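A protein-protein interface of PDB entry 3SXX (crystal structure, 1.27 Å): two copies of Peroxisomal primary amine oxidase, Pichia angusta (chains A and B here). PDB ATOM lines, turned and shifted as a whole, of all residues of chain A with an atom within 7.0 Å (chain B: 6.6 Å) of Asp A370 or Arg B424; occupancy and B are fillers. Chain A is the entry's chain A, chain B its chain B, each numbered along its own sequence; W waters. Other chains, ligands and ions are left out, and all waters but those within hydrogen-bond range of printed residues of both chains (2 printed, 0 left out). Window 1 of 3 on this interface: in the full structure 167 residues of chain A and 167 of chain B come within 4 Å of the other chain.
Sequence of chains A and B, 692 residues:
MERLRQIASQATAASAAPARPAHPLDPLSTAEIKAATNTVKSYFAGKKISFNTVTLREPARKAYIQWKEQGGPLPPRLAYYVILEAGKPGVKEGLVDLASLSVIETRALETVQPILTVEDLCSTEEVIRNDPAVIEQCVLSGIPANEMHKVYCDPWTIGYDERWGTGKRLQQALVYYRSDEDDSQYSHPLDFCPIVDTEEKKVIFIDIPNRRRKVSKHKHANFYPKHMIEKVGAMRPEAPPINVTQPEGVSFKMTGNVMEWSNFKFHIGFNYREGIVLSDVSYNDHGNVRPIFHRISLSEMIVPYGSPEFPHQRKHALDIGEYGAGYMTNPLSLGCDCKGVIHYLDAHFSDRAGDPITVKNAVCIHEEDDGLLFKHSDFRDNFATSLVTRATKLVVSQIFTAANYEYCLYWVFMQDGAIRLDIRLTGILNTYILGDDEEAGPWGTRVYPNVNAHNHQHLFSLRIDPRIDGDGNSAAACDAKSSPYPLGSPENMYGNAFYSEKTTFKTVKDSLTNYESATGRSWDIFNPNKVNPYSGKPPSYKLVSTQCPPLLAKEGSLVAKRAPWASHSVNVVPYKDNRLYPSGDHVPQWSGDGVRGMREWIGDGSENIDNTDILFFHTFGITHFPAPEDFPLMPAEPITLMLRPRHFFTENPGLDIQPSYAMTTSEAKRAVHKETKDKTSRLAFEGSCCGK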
ATOM      1  N   GLU A 368      29.755  22.975   9.174  1.00  0.00           N
ATOM      2  CA  GLU A 368      29.092  21.741   9.665  1.00  0.00           C
ATOM      3  C   GLU A 368      28.210  22.142  10.853  1.00  0.00           C
ATOM      4  O   GLU A 368      28.565  23.049  11.634  1.00  0.00           O
ATOM      5  CB  GLU A 368      30.175  20.763  10.238  1.00  0.00           C
ATOM      6  CG  GLU A 368      31.180  20.050   9.263  1.00  0.00           C
ATOM      7  CD  GLU A 368      31.893  18.914  10.022  1.00  0.00           C
ATOM      8  OE1 GLU A 368      31.206  18.238  10.851  1.00  0.00           O
ATOM      9  OE2 GLU A 368      33.137  18.882   9.984  1.00  0.00           O
ATOM     10  N   ASP A 369      27.107  21.428  11.007  1.00  0.00           N
ATOM     11  CA  ASP A 369      26.333  21.375  12.262  1.00  0.00           C
ATOM     12  C   ASP A 369      27.217  21.108  13.451  1.00  0.00           C
ATOM     13  O   ASP A 369      28.103  20.241  13.363  1.00  0.00           O
ATOM     14  CB  ASP A 369      25.403  20.167  12.222  1.00  0.00           C
ATOM     15  CG  ASP A 369      24.285  20.336  11.240  1.00  0.00           C
ATOM     16  OD1 ASP A 369      24.012  21.508  10.924  1.00  0.00           O
ATOM     17  OD2 ASP A 369      23.553  19.337  10.945  1.00  0.00           O
ATOM     18  N   ASP A 370      27.081  21.857  14.525  1.00  0.00           N
ATOM     19  CA  ASP A 370      27.841  21.534  15.704  1.00  0.00           C
ATOM     20  C   ASP A 370      26.915  21.520  16.948  1.00  0.00           C
ATOM     21  O   ASP A 370      27.339  21.952  17.987  1.00  0.00           O
ATOM     22  CB  ASP A 370      28.982  22.533  15.894  1.00  0.00           C
ATOM     23  CG  ASP A 370      30.011  22.025  16.864  1.00  0.00           C
ATOM     24  OD1 ASP A 370      29.987  20.776  17.096  1.00  0.00           O
ATOM     25  OD2 ASP A 370      30.760  22.844  17.435  1.00  0.00           O
ATOM     26  N   GLY A 371      25.677  21.035  16.823  1.00  0.00           N
ATOM     27  CA  GLY A 371      24.829  20.836  18.006  1.00  0.00           C
ATOM     28  C   GLY A 371      24.307  22.174  18.470  1.00  0.00           C
ATOM     29  O   GLY A 371      23.984  23.018  17.648  1.00  0.00           O
ATOM     30  N   LEU A 372      24.118  22.315  19.792  1.00  0.00           N
ATOM     31  CA  LEU A 372      23.539  23.514  20.326  1.00  0.00           C
ATOM     32  C   LEU A 372      24.553  24.602  20.608  1.00  0.00           C
ATOM     33  O   LEU A 372      25.643  24.313  21.134  1.00  0.00           O
ATOM     34  CB  LEU A 372      22.834  23.215  21.675  1.00  0.00           C
ATOM     35  CG  LEU A 372      21.599  22.316  21.485  1.00  0.00           C
ATOM     36  CD1 LEU A 372      20.883  22.155  22.821  1.00  0.00           C
ATOM     37  CD2 LEU A 372      20.647  22.736  20.326  1.00  0.00           C
ATOM     38  N   LEU A 373      24.211  25.853  20.300  1.00  0.00           N
ATOM     39  CA  LEU A 373      25.034  26.992  20.687  1.00  0.00           C
ATOM     40  C   LEU A 373      24.628  27.474  22.074  1.00  0.00           C
ATOM     41  O   LEU A 373      25.485  27.715  22.939  1.00  0.00           O
ATOM     42  CB  LEU A 373      24.919  28.100  19.647  1.00  0.00           C
ATOM     43  CG  LEU A 373      25.958  29.236  19.737  1.00  0.00           C
ATOM     44  CD1 LEU A 373      27.407  28.710  19.613  1.00  0.00           C
ATOM     45  CD2 LEU A 373      25.698  30.291  18.681  1.00  0.00           C
ATOM     46  N   ARG A 390      20.993  26.805  17.446  1.00  0.00           N
ATOM     47  CA  ARG A 390      21.932  25.762  17.013  1.00  0.00           C
ATOM     48  C   ARG A 390      23.246  26.407  16.574  1.00  0.00           C
ATOM     49  O   ARG A 390      23.280  27.543  16.127  1.00  0.00           O
ATOM     50  CB  ARG A 390      21.326  24.896  15.890  1.00  0.00           C
ATOM     51  CG  ARG A 390      20.166  24.032  16.428  1.00  0.00           C
ATOM     52  CD  ARG A 390      19.811  22.927  15.536  1.00  0.00           C
ATOM     53  NE  ARG A 390      20.861  21.909  15.430  1.00  0.00           N
ATOM     54  CZ  ARG A 390      21.055  20.896  16.275  1.00  0.00           C
ATOM     55  NH1 ARG A 390      20.207  20.636  17.260  1.00  0.00           N
ATOM     56  NH2 ARG A 390      22.120  20.116  16.109  1.00  0.00           N
ATOM     57  N   ALA A 391      24.320  25.645  16.734  1.00  0.00           N
ATOM     58  CA  ALA A 391      25.669  26.108  16.374  1.00  0.00           C
ATOM     59  C   ALA A 391      26.090  25.578  15.026  1.00  0.00           C
ATOM     60  O   ALA A 391      25.794  24.414  14.697  1.00  0.00           O
ATOM     61  CB  ALA A 391      26.634  25.518  17.388  1.00  0.00           C
ATOM     62  N   THR A 392      26.836  26.391  14.285  1.00  0.00           N
ATOM     63  CA  THR A 392      27.531  25.916  13.090  1.00  0.00           C
ATOM     64  C   THR A 392      29.017  26.176  13.325  1.00  0.00           C
ATOM     65  O   THR A 392      29.373  27.176  13.939  1.00  0.00           O
ATOM     66  CB  THR A 392      27.016  26.736  11.867  1.00  0.00           C
ATOM     67  OG1 THR A 392      25.607  26.553  11.767  1.00  0.00           O
ATOM     68  CG2 THR A 392      27.686  26.303  10.555  1.00  0.00           C
ATOM     69  N   LYS A 393      29.867  25.254  12.849  1.00  0.00           N
ATOM     70  CA  LYS A 393      31.308  25.457  12.937  1.00  0.00           C
ATOM     71  C   LYS A 393      31.910  25.548  11.526  1.00  0.00           C
ATOM     72  O   LYS A 393      31.381  24.881  10.584  1.00  0.00           O
ATOM     73  CB  LYS A 393      31.987  24.352  13.764  1.00  0.00           C
ATOM     74  CG  LYS A 393      31.883  22.947  13.174  1.00  0.00           C
ATOM     75  CD  LYS A 393      32.514  21.857  14.046  1.00  0.00           C
ATOM     76  CE  LYS A 393      32.249  20.462  13.537  1.00  0.00           C
ATOM     77  NZ  LYS A 393      32.960  19.453  14.405  1.00  0.00           N
ATOM     78  N   VAL A 412      39.108  24.872  13.663  1.00  0.00           N
ATOM     79  CA  VAL A 412      37.649  25.006  13.797  1.00  0.00           C
ATOM     80  C   VAL A 412      37.334  26.382  14.394  1.00  0.00           C
ATOM     81  O   VAL A 412      37.850  26.744  15.471  1.00  0.00           O
ATOM     82  CB  VAL A 412      37.129  23.889  14.720  1.00  0.00           C
ATOM     83  CG1 VAL A 412      35.632  24.061  14.898  1.00  0.00           C
ATOM     84  CG2 VAL A 412      37.485  22.510  14.146  1.00  0.00           C
ATOM     85  N   PHE A 413      36.493  27.139  13.709  1.00  0.00           N
ATOM     86  CA  PHE A 413      36.013  28.422  14.201  1.00  0.00           C
ATOM     87  C   PHE A 413      34.582  28.240  14.680  1.00  0.00           C
ATOM     88  O   PHE A 413      33.781  27.568  14.008  1.00  0.00           O
ATOM     89  CB  PHE A 413      36.124  29.488  13.106  1.00  0.00           C
ATOM     90  CG  PHE A 413      37.547  29.837  12.772  1.00  0.00           C
ATOM     91  CD1 PHE A 413      38.351  28.976  12.029  1.00  0.00           C
ATOM     92  CD2 PHE A 413      38.088  31.046  13.239  1.00  0.00           C
ATOM     93  CE1 PHE A 413      39.728  29.285  11.783  1.00  0.00           C
ATOM     94  CE2 PHE A 413      39.420  31.355  12.977  1.00  0.00           C
ATOM     95  CZ  PHE A 413      40.226  30.486  12.261  1.00  0.00           C
ATOM     96  N   MET A 414      34.214  28.881  15.786  1.00  0.00           N
ATOM     97  CA  MET A 414      32.872  28.669  16.333  1.00  0.00           C
ATOM     98  C   MET A 414      32.198  29.997  16.622  1.00  0.00           C
ATOM     99  O   MET A 414      32.801  31.075  16.663  1.00  0.00           O
ATOM    100  CB  MET A 414      32.884  27.740  17.585  1.00  0.00           C
ATOM    101  CG  MET A 414      33.151  26.222  17.237  1.00  0.00           C
ATOM    102  SD  MET A 414      33.544  25.218  18.672  1.00  0.00           S
ATOM    103  CE  MET A 414      34.843  26.297  19.301  1.00  0.00           C
ATOM    104  N   ARG A 420      39.265  26.363  17.861  1.00  0.00           N
ATOM    105  CA  ARG A 420      39.746  25.079  18.387  1.00  0.00           C
ATOM    106  C   ARG A 420      40.651  24.418  17.355  1.00  0.00           C
ATOM    107  O   ARG A 420      40.434  24.590  16.148  1.00  0.00           O
ATOM    108  CB  ARG A 420      38.515  24.198  18.698  1.00  0.00           C
ATOM    109  CG  ARG A 420      38.718  22.911  19.351  1.00  0.00           C
ATOM    110  CD  ARG A 420      37.260  22.369  19.627  1.00  0.00           C
ATOM    111  NE  ARG A 420      36.634  21.754  18.478  1.00  0.00           N
ATOM    112  CZ  ARG A 420      35.344  21.512  18.361  1.00  0.00           C
ATOM    113  NH1 ARG A 420      34.584  21.896  19.425  1.00  0.00           N
ATOM    114  NH2 ARG A 420      34.811  20.844  17.270  1.00  0.00           N
ATOM    115  N   GLU B 406      21.087  24.916  32.212  1.00  0.00           N
ATOM    116  CA  GLU B 406      20.693  23.809  31.345  1.00  0.00           C
ATOM    117  C   GLU B 406      21.846  22.851  31.258  1.00  0.00           C
ATOM    118  O   GLU B 406      22.973  23.245  30.968  1.00  0.00           O
ATOM    119  CB  GLU B 406      20.296  24.294  29.942  1.00  0.00           C
ATOM    120  CG  GLU B 406      18.786  24.422  29.804  1.00  0.00           C
ATOM    121  CD  GLU B 406      18.152  25.680  30.365  1.00  0.00           C
ATOM    122  OE1 GLU B 406      16.883  25.727  30.347  1.00  0.00           O
ATOM    123  OE2 GLU B 406      18.884  26.602  30.774  1.00  0.00           O
ATOM    124  N   TYR B 407      21.566  21.574  31.460  1.00  0.00           N
ATOM    125  CA  TYR B 407      22.559  20.516  31.309  1.00  0.00           C
ATOM    126  C   TYR B 407      22.120  19.613  30.161  1.00  0.00           C
ATOM    127  O   TYR B 407      21.075  18.948  30.226  1.00  0.00           O
ATOM    128  CB  TYR B 407      22.656  19.697  32.631  1.00  0.00           C
ATOM    129  CG  TYR B 407      23.236  20.484  33.750  1.00  0.00           C
ATOM    130  CD1 TYR B 407      22.419  21.292  34.535  1.00  0.00           C
ATOM    131  CD2 TYR B 407      24.612  20.427  34.023  1.00  0.00           C
ATOM    132  CE1 TYR B 407      22.969  22.048  35.606  1.00  0.00           C
ATOM    133  CE2 TYR B 407      25.159  21.189  35.072  1.00  0.00           C
ATOM    134  CZ  TYR B 407      24.347  21.966  35.849  1.00  0.00           C
ATOM    135  OH  TYR B 407      24.886  22.703  36.862  1.00  0.00           O
ATOM    136  N   CYS B 408      22.958  19.564  29.106  1.00  0.00           N
ATOM    137  CA  CYS B 408      22.646  18.792  27.926  1.00  0.00           C
ATOM    138  C   CYS B 408      23.520  17.559  27.984  1.00  0.00           C
ATOM    139  O   CYS B 408      24.777  17.654  28.034  1.00  0.00           O
ATOM    140  CB  CYS B 408      22.965  19.547  26.620  1.00  0.00           C
ATOM    141  SG  CYS B 408      22.207  21.215  26.596  1.00  0.00           S
ATOM    142  N   LEU B 409      22.921  16.374  28.069  1.00  0.00           N
ATOM    143  CA  LEU B 409      23.635  15.104  28.280  1.00  0.00           C
ATOM    144  C   LEU B 409      23.569  14.229  27.079  1.00  0.00           C
ATOM    145  O   LEU B 409      22.463  13.989  26.555  1.00  0.00           O
ATOM    146  CB  LEU B 409      23.029  14.360  29.506  1.00  0.00           C
ATOM    147  CG  LEU B 409      22.855  15.197  30.782  1.00  0.00           C
ATOM    148  CD1 LEU B 409      22.203  14.385  31.858  1.00  0.00           C
ATOM    149  CD2 LEU B 409      24.103  15.780  31.267  1.00  0.00           C
ATOM    150  N   TYR B 410      24.707  13.701  26.637  1.00  0.00           N
ATOM    151  CA  TYR B 410      24.757  12.919  25.403  1.00  0.00           C
ATOM    152  C   TYR B 410      25.578  11.680  25.687  1.00  0.00           C
ATOM    153  O   TYR B 410      26.802  11.757  25.859  1.00  0.00           O
ATOM    154  CB  TYR B 410      25.400  13.698  24.272  1.00  0.00           C
ATOM    155  CG  TYR B 410      24.815  15.065  23.975  1.00  0.00           C
ATOM    156  CD1 TYR B 410      25.291  16.207  24.616  1.00  0.00           C
ATOM    157  CD2 TYR B 410      23.783  15.199  23.034  1.00  0.00           C
ATOM    158  CE1 TYR B 410      24.724  17.442  24.404  1.00  0.00           C
ATOM    159  CE2 TYR B 410      23.229  16.442  22.758  1.00  0.00           C
ATOM    160  CZ  TYR B 410      23.689  17.553  23.442  1.00  0.00           C
ATOM    161  OH  TYR B 410      23.094  18.786  23.183  1.00  0.00           O
ATOM    162  N   ASP B 422      29.273  12.984  26.708  1.00  0.00           N
ATOM    163  CA  ASP B 422      29.503  14.389  26.426  1.00  0.00           C
ATOM    164  C   ASP B 422      28.434  15.214  27.135  1.00  0.00           C
ATOM    165  O   ASP B 422      27.256  14.838  27.101  1.00  0.00           O
ATOM    166  CB  ASP B 422      29.359  14.680  24.921  1.00  0.00           C
ATOM    167  CG  ASP B 422      30.431  14.072  24.041  1.00  0.00           C
ATOM    168  OD1 ASP B 422      31.523  13.774  24.534  1.00  0.00           O
ATOM    169  OD2 ASP B 422      30.216  13.883  22.829  1.00  0.00           O
ATOM    170  N   ILE B 423      28.831  16.291  27.781  1.00  0.00           N
ATOM    171  CA  ILE B 423      27.913  17.213  28.407  1.00  0.00           C
ATOM    172  C   ILE B 423      28.144  18.604  27.786  1.00  0.00           C
ATOM    173  O   ILE B 423      29.308  18.984  27.527  1.00  0.00           O
ATOM    174  CB  ILE B 423      28.122  17.226  29.940  1.00  0.00           C
ATOM    175  CG1 ILE B 423      27.842  15.837  30.529  1.00  0.00           C
ATOM    176  CG2 ILE B 423      27.294  18.341  30.588  1.00  0.00           C
ATOM    177  CD1 ILE B 423      27.981  15.735  32.027  1.00  0.00           C
ATOM    178  N   ARG B 424      27.066  19.337  27.563  1.00  0.00           N
ATOM    179  CA  ARG B 424      27.171  20.763  27.258  1.00  0.00           C
ATOM    180  C   ARG B 424      26.397  21.519  28.308  1.00  0.00           C
ATOM    181  O   ARG B 424      25.216  21.241  28.521  1.00  0.00           O
ATOM    182  CB  ARG B 424      26.660  21.080  25.877  1.00  0.00           C
ATOM    183  CG  ARG B 424      27.497  20.460  24.793  1.00  0.00           C
ATOM    184  CD  ARG B 424      27.093  21.026  23.452  1.00  0.00           C
ATOM    185  NE  ARG B 424      27.855  20.353  22.389  1.00  0.00           N
ATOM    186  CZ  ARG B 424      27.894  20.788  21.132  1.00  0.00           C
ATOM    187  NH1 ARG B 424      27.259  21.901  20.753  1.00  0.00           N
ATOM    188  NH2 ARG B 424      28.544  20.071  20.230  1.00  0.00           N
ATOM    189  N   LEU B 425      27.075  22.456  28.971  1.00  0.00           N
ATOM    190  CA  LEU B 425      26.430  23.374  29.935  1.00  0.00           C
ATOM    191  C   LEU B 425      25.972  24.620  29.188  1.00  0.00           C
ATOM    192  O   LEU B 425      26.795  25.262  28.546  1.00  0.00           O
ATOM    193  CB  LEU B 425      27.447  23.798  30.995  1.00  0.00           C
ATOM    194  CG  LEU B 425      28.125  22.654  31.747  1.00  0.00           C
ATOM    195  CD1 LEU B 425      28.981  23.186  32.840  1.00  0.00           C
ATOM    196  CD2 LEU B 425      27.091  21.678  32.325  1.00  0.00           C
ATOM    197  N   THR B 426      24.726  25.029  29.426  1.00  0.00           N
ATOM    198  CA  THR B 426      24.259  26.310  28.871  1.00  0.00           C
ATOM    199  C   THR B 426      23.225  26.856  29.853  1.00  0.00           C
ATOM    200  O   THR B 426      23.262  26.504  31.047  1.00  0.00           O
ATOM    201  CB  THR B 426      23.810  26.127  27.407  1.00  0.00           C
ATOM    202  OG1 THR B 426      23.419  27.393  26.875  1.00  0.00           O
ATOM    203  CG2 THR B 426      22.648  25.161  27.219  1.00  0.00           C
ATOM    204  N   ALA B 636      27.352  27.277  25.021  1.00  0.00           N
ATOM    205  CA  ALA B 636      27.588  25.910  25.543  1.00  0.00           C
ATOM    206  C   ALA B 636      29.056  25.693  25.879  1.00  0.00           C
ATOM    207  O   ALA B 636      29.945  26.003  25.075  1.00  0.00           O
ATOM    208  CB  ALA B 636      27.174  24.897  24.521  1.00  0.00           C
ATOM    209  N   GLU B 637      29.285  25.133  27.046  1.00  0.00           N
ATOM    210  CA  GLU B 637      30.638  24.779  27.482  1.00  0.00           C
ATOM    211  C   GLU B 637      30.717  23.254  27.562  1.00  0.00           C
ATOM    212  O   GLU B 637      29.865  22.588  28.192  1.00  0.00           O
ATOM    213  CB  GLU B 637      30.960  25.330  28.869  1.00  0.00           C
ATOM    214  CG  GLU B 637      32.443  25.026  29.195  1.00  0.00           C
ATOM    215  CD  GLU B 637      32.984  25.694  30.440  1.00  0.00           C
ATOM    216  OE1 GLU B 637      32.293  26.503  31.043  1.00  0.00           O
ATOM    217  OE2 GLU B 637      34.096  25.271  30.923  1.00  0.00           O
ATOM    218  N   PRO B 638      31.716  22.625  26.937  1.00  0.00           N
ATOM    219  CA  PRO B 638      31.756  21.148  26.838  1.00  0.00           C
ATOM    220  C   PRO B 638      32.496  20.455  27.972  1.00  0.00           C
ATOM    221  O   PRO B 638      33.495  20.965  28.506  1.00  0.00           O
ATOM    222  CB  PRO B 638      32.532  20.910  25.511  1.00  0.00           C
ATOM    223  CG  PRO B 638      33.507  22.088  25.491  1.00  0.00           C
ATOM    224  CD  PRO B 638      32.715  23.298  26.062  1.00  0.00           C
ATOM    225  N   ILE B 639      32.039  19.263  28.268  1.00  0.00           N
ATOM    226  CA  ILE B 639      32.736  18.355  29.186  1.00  0.00           C
ATOM    227  C   ILE B 639      32.648  16.979  28.536  1.00  0.00           C
ATOM    228  O   ILE B 639      31.636  16.645  27.914  1.00  0.00           O
ATOM    229  CB  ILE B 639      32.047  18.276  30.586  1.00  0.00           C
ATOM    230  CG1 ILE B 639      31.556  19.671  31.008  1.00  0.00           C
ATOM    231  CG2 ILE B 639      33.027  17.668  31.577  1.00  0.00           C
ATOM    232  CD1 ILE B 639      30.812  19.649  32.356  1.00  0.00           C
HETATM  233  O   HOH W   1      28.455  25.123  20.860  1.00  0.00           O
HETATM  234  O   HOH W   2      24.682  19.943  21.334  1.00  0.00           O
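The side-chain carboxylate (OD1) of Asp A370 is in salt-bridge range of the guanidinium group (NH2) of Arg B424, 3.5 Å away.
NH1 of Arg B424 lies within hydrogen-bond range of O of Leu A372 (2.9 Å).
The backbone NH (N) of Ala B636 is in hydrogen-bond range of the backbone carbonyl oxygen (O) of Leu A373, at 2.8 Å.
The backbone NH (N) of Ala A391 sits at hydrogen-bond distance from the backbone carbonyl oxygen (O) of Gly A371, at 2.8 Å.
The backbone NH (N) of Asp A370 is in hydrogen-bond range of the backbone carbonyl oxygen (O) of Ala A391, at 2.9 Å.
O of Arg B424 lies within hydrogen-bond range of N of Cys B408 (2.9 Å).
Gly A371 touches Arg B424.
O of Leu A372 touches CB of Ala B636, 3.8 Å away.
Of chain B, only Arg B424 comes within 4 Å of Asp A370.
Printed residues of chain A within 4 Å of Arg B424: Asp A370, Gly A371 and Leu A372.
Printed residues of chain B within 4 Å of Leu A372: Arg B424 (2.9 Å) and Ala B636 (3.8 Å).
Printed residues of chain B within 4 Å of Leu A373: Ala B636.
Of the printed residues of chain B, Gly A371 touches Arg B424 (3.7 Å).
Of the printed residues of chain A, Ala B636 touches Leu A372 (3.8 Å) and Leu A373 (2.8 Å).
Glu A368 touches none of the printed residues of chain B.
The nearest printed residue of chain B that does not touch Asp A370 is Ala B636 (7.2 Å).
Of the 14 printed residues of chain B, 2 touch a printed residue of chain A.
Hydrophobic or aromatic side chains of chain B that line the printed part of chain A: Ala B636.
Of the 14 printed residues of chain A, 4 touch a printed residue of chain B.
Among the printed residues, 5 pairs touch across the chains.
Among the printed residues, Asp or Glu carboxylates within 4 Å of a Lys or Arg side-chain nitrogen of the other chain: Asp A370 with Arg B424.
No position is printed for both chains.
Water W2 lies within hydrogen-bond range of OH of Tyr B410 (2.7 Å), N of Leu A372 (2.9 Å) and NH1 of Arg B424 (3.3 Å).
Water W1 lies within hydrogen-bond range of O of Leu A372 and NH1 of Arg B424.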
